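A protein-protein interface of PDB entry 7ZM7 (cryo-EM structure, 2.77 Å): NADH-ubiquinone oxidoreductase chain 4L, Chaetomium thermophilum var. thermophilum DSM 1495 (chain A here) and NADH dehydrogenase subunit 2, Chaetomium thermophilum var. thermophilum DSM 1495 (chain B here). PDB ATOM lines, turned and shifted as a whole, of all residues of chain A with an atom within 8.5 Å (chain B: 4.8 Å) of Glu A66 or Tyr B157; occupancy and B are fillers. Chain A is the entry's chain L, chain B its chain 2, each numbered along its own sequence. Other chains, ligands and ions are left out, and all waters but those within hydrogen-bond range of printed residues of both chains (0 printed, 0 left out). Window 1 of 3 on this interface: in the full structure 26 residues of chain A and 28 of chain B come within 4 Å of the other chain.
The side-chain hydroxyl (OH) of Tyr B157 lies close to the side-chain carboxylate (OE1) of Glu A66 (3.0 Å).
OE2 of Glu B153 is in hydrogen-bond range of OH of Tyr B157 (2.9 Å).
Leu A26 touches Phe B180.
Gly B184 touches Ile A29 (C to CD1, 3.97 Å).
Glu B153 touches Val A62 (OE2 to CG1, 3.5 Å).
OH of Tyr B157 touches CG1 of Val A62 (3.5 Å).
Glu A66 touches Phe B180 (O to CZ, 3.1 Å).
CD1 of Ile A69 touches CD1 of Leu B161, 3.8 Å away.
CZ of Phe B180 touches CA of Gly A70, 3.3 Å away.
Ile A73 touches Tyr B160 (CD1 to CB, 3.96 Å).
Glu A66 touches just these residues of chain B: Tyr B157 (2.9 Å) and Phe B180 (3.1 Å).
Ser A67 touches none of the printed residues of chain B.
Printed residues of chain B within 4 Å of Ile A73: Tyr B160 (3.96 Å).
Tyr B157 touches just these residues of chain A: Val A62 and Glu A66.
No residue of chain A comes within 4 Å of Gly B158.
Printed residues of chain A within 4 Å of Gly B184: Ile A29.
The nearest residue of chain B that does not touch Glu A66 is Glu B153 (4.1 Å).
The nearest residue of chain A that does not touch Tyr B157 is Ile A69 (4.6 Å).
Hydrophobic or aromatic side chains of chain B that line the printed part of chain A: Tyr B157, Tyr B160, Leu B161 and Phe B180.
Along chain B the printed residues that touch a printed residue of chain A span positions 153 to 184.
Of the 23 printed residues of chain A, 7 touch a printed residue of chain B.
Hydrophobic or aromatic side chains of chain A that line the printed part of chain B: Leu A26, Ile A29, Val A62, Ile A69 and Ile A73.
Among the printed residues, no Asp or Glu carboxylate lies within 4 Å of a Lys or Arg side-chain nitrogen of the other chain.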
ATOM      1  N   MET A  25     -29.192   2.449  20.329  1.00  0.00           N
ATOM      2  CA  MET A  25     -28.824   3.858  20.234  1.00  0.00           C
ATOM      3  C   MET A  25     -27.911   4.118  19.040  1.00  0.00           C
ATOM      4  O   MET A  25     -28.022   5.150  18.378  1.00  0.00           O
ATOM      5  CB  MET A  25     -28.190   4.370  21.517  1.00  0.00           C
ATOM      6  CG  MET A  25     -29.198   4.817  22.530  1.00  0.00           C
ATOM      7  SD  MET A  25     -28.425   5.838  23.775  1.00  0.00           S
ATOM      8  CE  MET A  25     -27.193   4.697  24.328  1.00  0.00           C
ATOM      9  N   LEU A  26     -27.017   3.189  18.742  1.00  0.00           N
ATOM     10  CA  LEU A  26     -26.256   3.265  17.502  1.00  0.00           C
ATOM     11  C   LEU A  26     -27.164   3.213  16.281  1.00  0.00           C
ATOM     12  O   LEU A  26     -26.933   3.916  15.295  1.00  0.00           O
ATOM     13  CB  LEU A  26     -25.241   2.131  17.465  1.00  0.00           C
ATOM     14  CG  LEU A  26     -24.055   2.433  18.354  1.00  0.00           C
ATOM     15  CD1 LEU A  26     -23.099   1.271  18.370  1.00  0.00           C
ATOM     16  CD2 LEU A  26     -23.405   3.631  17.765  1.00  0.00           C
ATOM     17  N   SER A  28     -30.585   3.908  15.944  1.00  0.00           N
ATOM     18  CA  SER A  28     -31.563   5.019  15.782  1.00  0.00           C
ATOM     19  C   SER A  28     -30.918   6.315  15.281  1.00  0.00           C
ATOM     20  O   SER A  28     -31.619   7.071  14.618  1.00  0.00           O
ATOM     21  CB  SER A  28     -32.383   5.191  17.017  1.00  0.00           C
ATOM     22  OG  SER A  28     -33.175   4.041  17.251  1.00  0.00           O
ATOM     23  N   ILE A  29     -29.648   6.556  15.607  1.00  0.00           N
ATOM     24  CA  ILE A  29     -28.913   7.737  15.081  1.00  0.00           C
ATOM     25  C   ILE A  29     -28.872   7.629  13.559  1.00  0.00           C
ATOM     26  O   ILE A  29     -29.039   8.661  12.883  1.00  0.00           O
ATOM     27  CB  ILE A  29     -27.508   7.832  15.706  1.00  0.00           C
ATOM     28  CG1 ILE A  29     -27.566   8.297  17.163  1.00  0.00           C
ATOM     29  CG2 ILE A  29     -26.585   8.714  14.878  1.00  0.00           C
ATOM     30  CD1 ILE A  29     -26.245   8.200  17.890  1.00  0.00           C
ATOM     31  N   GLU A  30     -28.739   6.414  13.042  1.00  0.00           N
ATOM     32  CA  GLU A  30     -28.619   6.219  11.583  1.00  0.00           C
ATOM     33  C   GLU A  30     -30.006   6.271  10.957  1.00  0.00           C
ATOM     34  O   GLU A  30     -30.104   6.719   9.809  1.00  0.00           O
ATOM     35  CB  GLU A  30     -27.966   4.867  11.328  1.00  0.00           C
ATOM     36  CG  GLU A  30     -26.472   4.964  11.099  1.00  0.00           C
ATOM     37  CD  GLU A  30     -25.950   3.942  10.104  1.00  0.00           C
ATOM     38  OE1 GLU A  30     -26.424   2.792  10.142  1.00  0.00           O
ATOM     39  OE2 GLU A  30     -25.085   4.307   9.285  1.00  0.00           O
ATOM     40  N   LEU A  33     -30.488   9.976  10.585  1.00  0.00           N
ATOM     41  CA  LEU A  33     -29.681  10.476   9.439  1.00  0.00           C
ATOM     42  C   LEU A  33     -30.370  10.124   8.123  1.00  0.00           C
ATOM     43  O   LEU A  33     -30.332  10.977   7.242  1.00  0.00           O
ATOM     44  CB  LEU A  33     -28.259   9.925   9.526  1.00  0.00           C
ATOM     45  CG  LEU A  33     -27.495  10.292  10.798  1.00  0.00           C
ATOM     46  CD1 LEU A  33     -26.159   9.575  10.866  1.00  0.00           C
ATOM     47  CD2 LEU A  33     -27.299  11.794  10.903  1.00  0.00           C
ATOM     48  N   TYR A  58     -22.569  13.802   0.923  1.00  0.00           N
ATOM     49  CA  TYR A  58     -21.649  14.070   2.015  1.00  0.00           C
ATOM     50  C   TYR A  58     -22.245  13.699   3.369  1.00  0.00           C
ATOM     51  O   TYR A  58     -21.491  13.438   4.311  1.00  0.00           O
ATOM     52  CB  TYR A  58     -21.233  15.535   1.993  1.00  0.00           C
ATOM     53  CG  TYR A  58     -20.285  15.864   0.867  1.00  0.00           C
ATOM     54  CD1 TYR A  58     -19.056  15.234   0.761  1.00  0.00           C
ATOM     55  CD2 TYR A  58     -20.617  16.803  -0.081  1.00  0.00           C
ATOM     56  CE1 TYR A  58     -18.203  15.529  -0.254  1.00  0.00           C
ATOM     57  CE2 TYR A  58     -19.770  17.099  -1.097  1.00  0.00           C
ATOM     58  CZ  TYR A  58     -18.566  16.466  -1.187  1.00  0.00           C
ATOM     59  OH  TYR A  58     -17.723  16.787  -2.219  1.00  0.00           O
ATOM     60  N   ILE A  59     -23.575  13.675   3.498  1.00  0.00           N
ATOM     61  CA  ILE A  59     -24.173  13.162   4.728  1.00  0.00           C
ATOM     62  C   ILE A  59     -23.976  11.661   4.819  1.00  0.00           C
ATOM     63  O   ILE A  59     -23.685  11.121   5.889  1.00  0.00           O
ATOM     64  CB  ILE A  59     -25.665  13.523   4.828  1.00  0.00           C
ATOM     65  CG1 ILE A  59     -25.874  15.016   4.933  1.00  0.00           C
ATOM     66  CG2 ILE A  59     -26.282  12.903   6.062  1.00  0.00           C
ATOM     67  CD1 ILE A  59     -27.269  15.404   4.603  1.00  0.00           C
ATOM     68  N   ILE A  60     -24.141  10.963   3.697  1.00  0.00           N
ATOM     69  CA  ILE A  60     -23.903   9.529   3.650  1.00  0.00           C
ATOM     70  C   ILE A  60     -22.450   9.218   3.967  1.00  0.00           C
ATOM     71  O   ILE A  60     -22.149   8.213   4.613  1.00  0.00           O
ATOM     72  CB  ILE A  60     -24.329   8.986   2.271  1.00  0.00           C
ATOM     73  CG1 ILE A  60     -25.833   9.180   2.051  1.00  0.00           C
ATOM     74  CG2 ILE A  60     -23.999   7.540   2.124  1.00  0.00           C
ATOM     75  CD1 ILE A  60     -26.273   9.055   0.614  1.00  0.00           C
ATOM     76  N   VAL A  61     -21.512  10.101   3.630  1.00  0.00           N
ATOM     77  CA  VAL A  61     -20.083   9.717   3.804  1.00  0.00           C
ATOM     78  C   VAL A  61     -19.737   9.951   5.276  1.00  0.00           C
ATOM     79  O   VAL A  61     -19.036   9.112   5.851  1.00  0.00           O
ATOM     80  CB  VAL A  61     -19.218  10.602   2.885  1.00  0.00           C
ATOM     81  CG1 VAL A  61     -17.757  10.646   3.284  1.00  0.00           C
ATOM     82  CG2 VAL A  61     -19.380  10.251   1.416  1.00  0.00           C
ATOM     83  N   VAL A  62     -20.209  11.049   5.858  1.00  0.00           N
ATOM     84  CA  VAL A  62     -20.022  11.326   7.308  1.00  0.00           C
ATOM     85  C   VAL A  62     -20.782  10.273   8.131  1.00  0.00           C
ATOM     86  O   VAL A  62     -20.289   9.873   9.190  1.00  0.00           O
ATOM     87  CB  VAL A  62     -20.401  12.784   7.651  1.00  0.00           C
ATOM     88  CG1 VAL A  62     -20.732  12.980   9.117  1.00  0.00           C
ATOM     89  CG2 VAL A  62     -19.338  13.765   7.199  1.00  0.00           C
ATOM     90  N   ALA A  63     -21.939   9.829   7.660  1.00  0.00           N
ATOM     91  CA  ALA A  63     -22.705   8.796   8.386  1.00  0.00           C
ATOM     92  C   ALA A  63     -21.923   7.486   8.489  1.00  0.00           C
ATOM     93  O   ALA A  63     -21.945   6.884   9.575  1.00  0.00           O
ATOM     94  CB  ALA A  63     -24.015   8.566   7.693  1.00  0.00           C
ATOM     95  N   GLY A  64     -21.296   7.043   7.401  1.00  0.00           N
ATOM     96  CA  GLY A  64     -20.473   5.825   7.445  1.00  0.00           C
ATOM     97  C   GLY A  64     -19.293   6.007   8.368  1.00  0.00           C
ATOM     98  O   GLY A  64     -19.002   5.084   9.130  1.00  0.00           O
ATOM     99  N   ALA A  65     -18.649   7.168   8.321  1.00  0.00           N
ATOM    100  CA  ALA A  65     -17.488   7.451   9.193  1.00  0.00           C
ATOM    101  C   ALA A  65     -17.925   7.431  10.655  1.00  0.00           C
ATOM    102  O   ALA A  65     -17.152   6.958  11.488  1.00  0.00           O
ATOM    103  CB  ALA A  65     -16.851   8.752   8.808  1.00  0.00           C
ATOM    104  N   GLU A  66     -19.118   7.922  10.997  1.00  0.00           N
ATOM    105  CA  GLU A  66     -19.506   7.803  12.431  1.00  0.00           C
ATOM    106  C   GLU A  66     -19.702   6.338  12.792  1.00  0.00           C
ATOM    107  O   GLU A  66     -19.366   5.980  13.918  1.00  0.00           O
ATOM    108  CB  GLU A  66     -20.700   8.649  12.877  1.00  0.00           C
ATOM    109  CG  GLU A  66     -21.972   8.512  12.077  1.00  0.00           C
ATOM    110  CD  GLU A  66     -22.937   9.640  12.392  1.00  0.00           C
ATOM    111  OE1 GLU A  66     -23.120  10.518  11.526  1.00  0.00           O
ATOM    112  OE2 GLU A  66     -23.478   9.655  13.513  1.00  0.00           O
ATOM    113  N   SER A  67     -20.217   5.532  11.867  1.00  0.00           N
ATOM    114  CA  SER A  67     -20.327   4.084  12.157  1.00  0.00           C
ATOM    115  C   SER A  67     -18.960   3.449  12.444  1.00  0.00           C
ATOM    116  O   SER A  67     -18.882   2.677  13.404  1.00  0.00           O
ATOM    117  CB  SER A  67     -20.998   3.433  11.016  1.00  0.00           C
ATOM    118  OG  SER A  67     -22.201   4.117  10.703  1.00  0.00           O
ATOM    119  N   ALA A  68     -17.925   3.793  11.679  1.00  0.00           N
ATOM    120  CA  ALA A  68     -16.571   3.254  11.923  1.00  0.00           C
ATOM    121  C   ALA A  68     -16.062   3.700  13.282  1.00  0.00           C
ATOM    122  O   ALA A  68     -15.556   2.851  14.028  1.00  0.00           O
ATOM    123  CB  ALA A  68     -15.617   3.772  10.876  1.00  0.00           C
ATOM    124  N   ILE A  69     -16.199   4.987  13.580  1.00  0.00           N
ATOM    125  CA  ILE A  69     -15.717   5.532  14.879  1.00  0.00           C
ATOM    126  C   ILE A  69     -16.573   4.930  15.995  1.00  0.00           C
ATOM    127  O   ILE A  69     -16.011   4.566  17.019  1.00  0.00           O
ATOM    128  CB  ILE A  69     -15.718   7.076  14.821  1.00  0.00           C
ATOM    129  CG1 ILE A  69     -14.752   7.600  13.759  1.00  0.00           C
ATOM    130  CG2 ILE A  69     -15.426   7.683  16.184  1.00  0.00           C
ATOM    131  CD1 ILE A  69     -13.331   7.160  13.975  1.00  0.00           C
ATOM    132  N   GLY A  70     -17.885   4.825  15.781  1.00  0.00           N
ATOM    133  CA  GLY A  70     -18.824   4.288  16.777  1.00  0.00           C
ATOM    134  C   GLY A  70     -18.653   2.818  17.077  1.00  0.00           C
ATOM    135  O   GLY A  70     -18.811   2.431  18.241  1.00  0.00           O
ATOM    136  N   LEU A  71     -18.412   2.017  16.037  1.00  0.00           N
ATOM    137  CA  LEU A  71     -18.212   0.570  16.243  1.00  0.00           C
ATOM    138  C   LEU A  71     -16.770   0.350  16.698  1.00  0.00           C
ATOM    139  O   LEU A  71     -16.546  -0.605  17.446  1.00  0.00           O
ATOM    140  CB  LEU A  71     -18.592  -0.187  14.973  1.00  0.00           C
ATOM    141  CG  LEU A  71     -20.093  -0.313  14.723  1.00  0.00           C
ATOM    142  CD1 LEU A  71     -20.369  -0.936  13.365  1.00  0.00           C
ATOM    143  CD2 LEU A  71     -20.760  -1.113  15.829  1.00  0.00           C
ATOM    144  N   GLY A  72     -15.847   1.228  16.309  1.00  0.00           N
ATOM    145  CA  GLY A  72     -14.504   1.099  16.841  1.00  0.00           C
ATOM    146  C   GLY A  72     -14.423   1.371  18.328  1.00  0.00           C
ATOM    147  O   GLY A  72     -13.722   0.665  19.058  1.00  0.00           O
ATOM    148  N   ILE A  73     -15.101   2.420  18.791  1.00  0.00           N
ATOM    149  CA  ILE A  73     -15.102   2.745  20.209  1.00  0.00           C
ATOM    150  C   ILE A  73     -15.862   1.687  20.987  1.00  0.00           C
ATOM    151  O   ILE A  73     -15.489   1.331  22.110  1.00  0.00           O
ATOM    152  CB  ILE A  73     -15.682   4.158  20.427  1.00  0.00           C
ATOM    153  CG1 ILE A  73     -14.673   5.213  19.998  1.00  0.00           C
ATOM    154  CG2 ILE A  73     -16.061   4.407  21.876  1.00  0.00           C
ATOM    155  CD1 ILE A  73     -15.230   6.594  19.957  1.00  0.00           C
ATOM    156  N   LEU A  74     -16.946   1.175  20.415  1.00  0.00           N
ATOM    157  CA  LEU A  74     -17.686   0.110  21.071  1.00  0.00           C
ATOM    158  C   LEU A  74     -16.862  -1.170  21.177  1.00  0.00           C
ATOM    159  O   LEU A  74     -17.095  -1.982  22.073  1.00  0.00           O
ATOM    160  CB  LEU A  74     -18.983  -0.156  20.327  1.00  0.00           C
ATOM    161  CG  LEU A  74     -19.882  -1.203  20.955  1.00  0.00           C
ATOM    162  CD1 LEU A  74     -20.789  -0.573  21.979  1.00  0.00           C
ATOM    163  CD2 LEU A  74     -20.652  -1.941  19.889  1.00  0.00           C
ATOM    164  N   GLU B 153     -18.463  17.971  12.501  1.00  0.00           N
ATOM    165  CA  GLU B 153     -18.140  16.518  12.547  1.00  0.00           C
ATOM    166  C   GLU B 153     -16.628  16.291  12.600  1.00  0.00           C
ATOM    167  O   GLU B 153     -16.190  15.513  13.449  1.00  0.00           O
ATOM    168  CB  GLU B 153     -18.724  15.800  11.329  1.00  0.00           C
ATOM    169  CG  GLU B 153     -20.238  15.892  11.248  1.00  0.00           C
ATOM    170  CD  GLU B 153     -21.027  15.336  12.423  1.00  0.00           C
ATOM    171  OE1 GLU B 153     -21.163  16.045  13.438  1.00  0.00           O
ATOM    172  OE2 GLU B 153     -21.524  14.200  12.311  1.00  0.00           O
ATOM    173  N   LEU B 154     -15.861  16.993  11.772  1.00  0.00           N
ATOM    174  CA  LEU B 154     -14.388  16.878  11.859  1.00  0.00           C
ATOM    175  C   LEU B 154     -13.943  17.169  13.290  1.00  0.00           C
ATOM    176  O   LEU B 154     -13.016  16.494  13.758  1.00  0.00           O
ATOM    177  CB  LEU B 154     -13.739  17.862  10.884  1.00  0.00           C
ATOM    178  CG  LEU B 154     -12.236  17.718  10.669  1.00  0.00           C
ATOM    179  CD1 LEU B 154     -11.843  16.259  10.488  1.00  0.00           C
ATOM    180  CD2 LEU B 154     -11.796  18.538   9.468  1.00  0.00           C
ATOM    181  N   GLN B 155     -14.543  18.142  13.982  1.00  0.00           N
ATOM    182  CA  GLN B 155     -14.060  18.487  15.346  1.00  0.00           C
ATOM    183  C   GLN B 155     -14.617  17.475  16.339  1.00  0.00           C
ATOM    184  O   GLN B 155     -13.858  17.021  17.200  1.00  0.00           O
ATOM    185  CB  GLN B 155     -14.480  19.892  15.769  1.00  0.00           C
ATOM    186  CG  GLN B 155     -13.718  20.405  16.977  1.00  0.00           C
ATOM    187  CD  GLN B 155     -14.300  21.667  17.558  1.00  0.00           C
ATOM    188  OE1 GLN B 155     -13.626  22.413  18.258  1.00  0.00           O
ATOM    189  NE2 GLN B 155     -15.563  21.920  17.267  1.00  0.00           N
ATOM    190  N   SER B 156     -15.893  17.131  16.200  1.00  0.00           N
ATOM    191  CA  SER B 156     -16.561  16.212  17.167  1.00  0.00           C
ATOM    192  C   SER B 156     -15.932  14.817  17.137  1.00  0.00           C
ATOM    193  O   SER B 156     -15.704  14.262  18.210  1.00  0.00           O
ATOM    194  CB  SER B 156     -18.031  16.145  16.876  1.00  0.00           C
ATOM    195  OG  SER B 156     -18.652  17.403  17.085  1.00  0.00           O
ATOM    196  N   TYR B 157     -15.732  14.253  15.948  1.00  0.00           N
ATOM    197  CA  TYR B 157     -15.180  12.887  15.777  1.00  0.00           C
ATOM    198  C   TYR B 157     -13.772  12.793  16.357  1.00  0.00           C
ATOM    199  O   TYR B 157     -13.415  11.722  16.850  1.00  0.00           O
ATOM    200  CB  TYR B 157     -15.249  12.440  14.310  1.00  0.00           C
ATOM    201  CG  TYR B 157     -16.639  12.204  13.787  1.00  0.00           C
ATOM    202  CD1 TYR B 157     -17.612  11.630  14.584  1.00  0.00           C
ATOM    203  CD2 TYR B 157     -16.976  12.537  12.487  1.00  0.00           C
ATOM    204  CE1 TYR B 157     -18.892  11.405  14.109  1.00  0.00           C
ATOM    205  CE2 TYR B 157     -18.251  12.319  11.996  1.00  0.00           C
ATOM    206  CZ  TYR B 157     -19.212  11.753  12.810  1.00  0.00           C
ATOM    207  OH  TYR B 157     -20.468  11.532  12.331  1.00  0.00           O
ATOM    208  N   GLY B 158     -13.012  13.878  16.297  1.00  0.00           N
ATOM    209  CA  GLY B 158     -11.627  13.839  16.793  1.00  0.00           C
ATOM    210  C   GLY B 158     -11.629  13.958  18.299  1.00  0.00           C
ATOM    211  O   GLY B 158     -10.717  13.410  18.916  1.00  0.00           O
ATOM    212  N   LEU B 159     -12.624  14.638  18.871  1.00  0.00           N
ATOM    213  CA  LEU B 159     -12.773  14.669  20.315  1.00  0.00           C
ATOM    214  C   LEU B 159     -13.127  13.299  20.875  1.00  0.00           C
ATOM    215  O   LEU B 159     -12.647  12.933  21.950  1.00  0.00           O
ATOM    216  CB  LEU B 159     -13.804  15.718  20.700  1.00  0.00           C
ATOM    217  CG  LEU B 159     -13.227  17.132  20.567  1.00  0.00           C
ATOM    218  CD1 LEU B 159     -14.265  18.165  20.843  1.00  0.00           C
ATOM    219  CD2 LEU B 159     -12.011  17.344  21.460  1.00  0.00           C
ATOM    220  N   TYR B 160     -13.961  12.528  20.171  1.00  0.00           N
ATOM    221  CA  TYR B 160     -14.284  11.176  20.624  1.00  0.00           C
ATOM    222  C   TYR B 160     -13.057  10.285  20.597  1.00  0.00           C
ATOM    223  O   TYR B 160     -12.861   9.457  21.488  1.00  0.00           O
ATOM    224  CB  TYR B 160     -15.384  10.545  19.767  1.00  0.00           C
ATOM    225  CG  TYR B 160     -16.628  11.362  19.596  1.00  0.00           C
ATOM    226  CD1 TYR B 160     -17.042  12.248  20.571  1.00  0.00           C
ATOM    227  CD2 TYR B 160     -17.388  11.255  18.446  1.00  0.00           C
ATOM    228  CE1 TYR B 160     -18.164  12.998  20.403  1.00  0.00           C
ATOM    229  CE2 TYR B 160     -18.511  12.005  18.271  1.00  0.00           C
ATOM    230  CZ  TYR B 160     -18.898  12.870  19.257  1.00  0.00           C
ATOM    231  OH  TYR B 160     -20.021  13.623  19.076  1.00  0.00           O
ATOM    232  N   LEU B 161     -12.230  10.430  19.571  1.00  0.00           N
ATOM    233  CA  LEU B 161     -11.040   9.605  19.445  1.00  0.00           C
ATOM    234  C   LEU B 161     -10.009   9.948  20.509  1.00  0.00           C
ATOM    235  O   LEU B 161      -9.298   9.070  20.999  1.00  0.00           O
ATOM    236  CB  LEU B 161     -10.459   9.770  18.052  1.00  0.00           C
ATOM    237  CG  LEU B 161     -11.338   9.126  16.995  1.00  0.00           C
ATOM    238  CD1 LEU B 161     -10.914   9.535  15.613  1.00  0.00           C
ATOM    239  CD2 LEU B 161     -11.329   7.613  17.152  1.00  0.00           C
ATOM    240  N   PHE B 180     -19.478   9.766  22.373  1.00  0.00           N
ATOM    241  CA  PHE B 180     -19.890   9.499  20.974  1.00  0.00           C
ATOM    242  C   PHE B 180     -21.399   9.308  20.892  1.00  0.00           C
ATOM    243  O   PHE B 180     -22.014   9.783  19.931  1.00  0.00           O
ATOM    244  CB  PHE B 180     -19.230   8.221  20.449  1.00  0.00           C
ATOM    245  CG  PHE B 180     -19.707   7.790  19.085  1.00  0.00           C
ATOM    246  CD1 PHE B 180     -19.069   8.236  17.941  1.00  0.00           C
ATOM    247  CD2 PHE B 180     -20.801   6.950  18.945  1.00  0.00           C
ATOM    248  CE1 PHE B 180     -19.521   7.858  16.689  1.00  0.00           C
ATOM    249  CE2 PHE B 180     -21.262   6.585  17.693  1.00  0.00           C
ATOM    250  CZ  PHE B 180     -20.621   7.042  16.568  1.00  0.00           C
ATOM    251  N   GLY B 184     -23.419  12.001  18.961  1.00  0.00           N
ATOM    252  CA  GLY B 184     -24.103  11.628  17.710  1.00  0.00           C
ATOM    253  C   GLY B 184     -25.532  12.104  17.680  1.00  0.00           C
ATOM    254  O   GLY B 184     -26.013  12.492  16.609  1.00  0.00           O
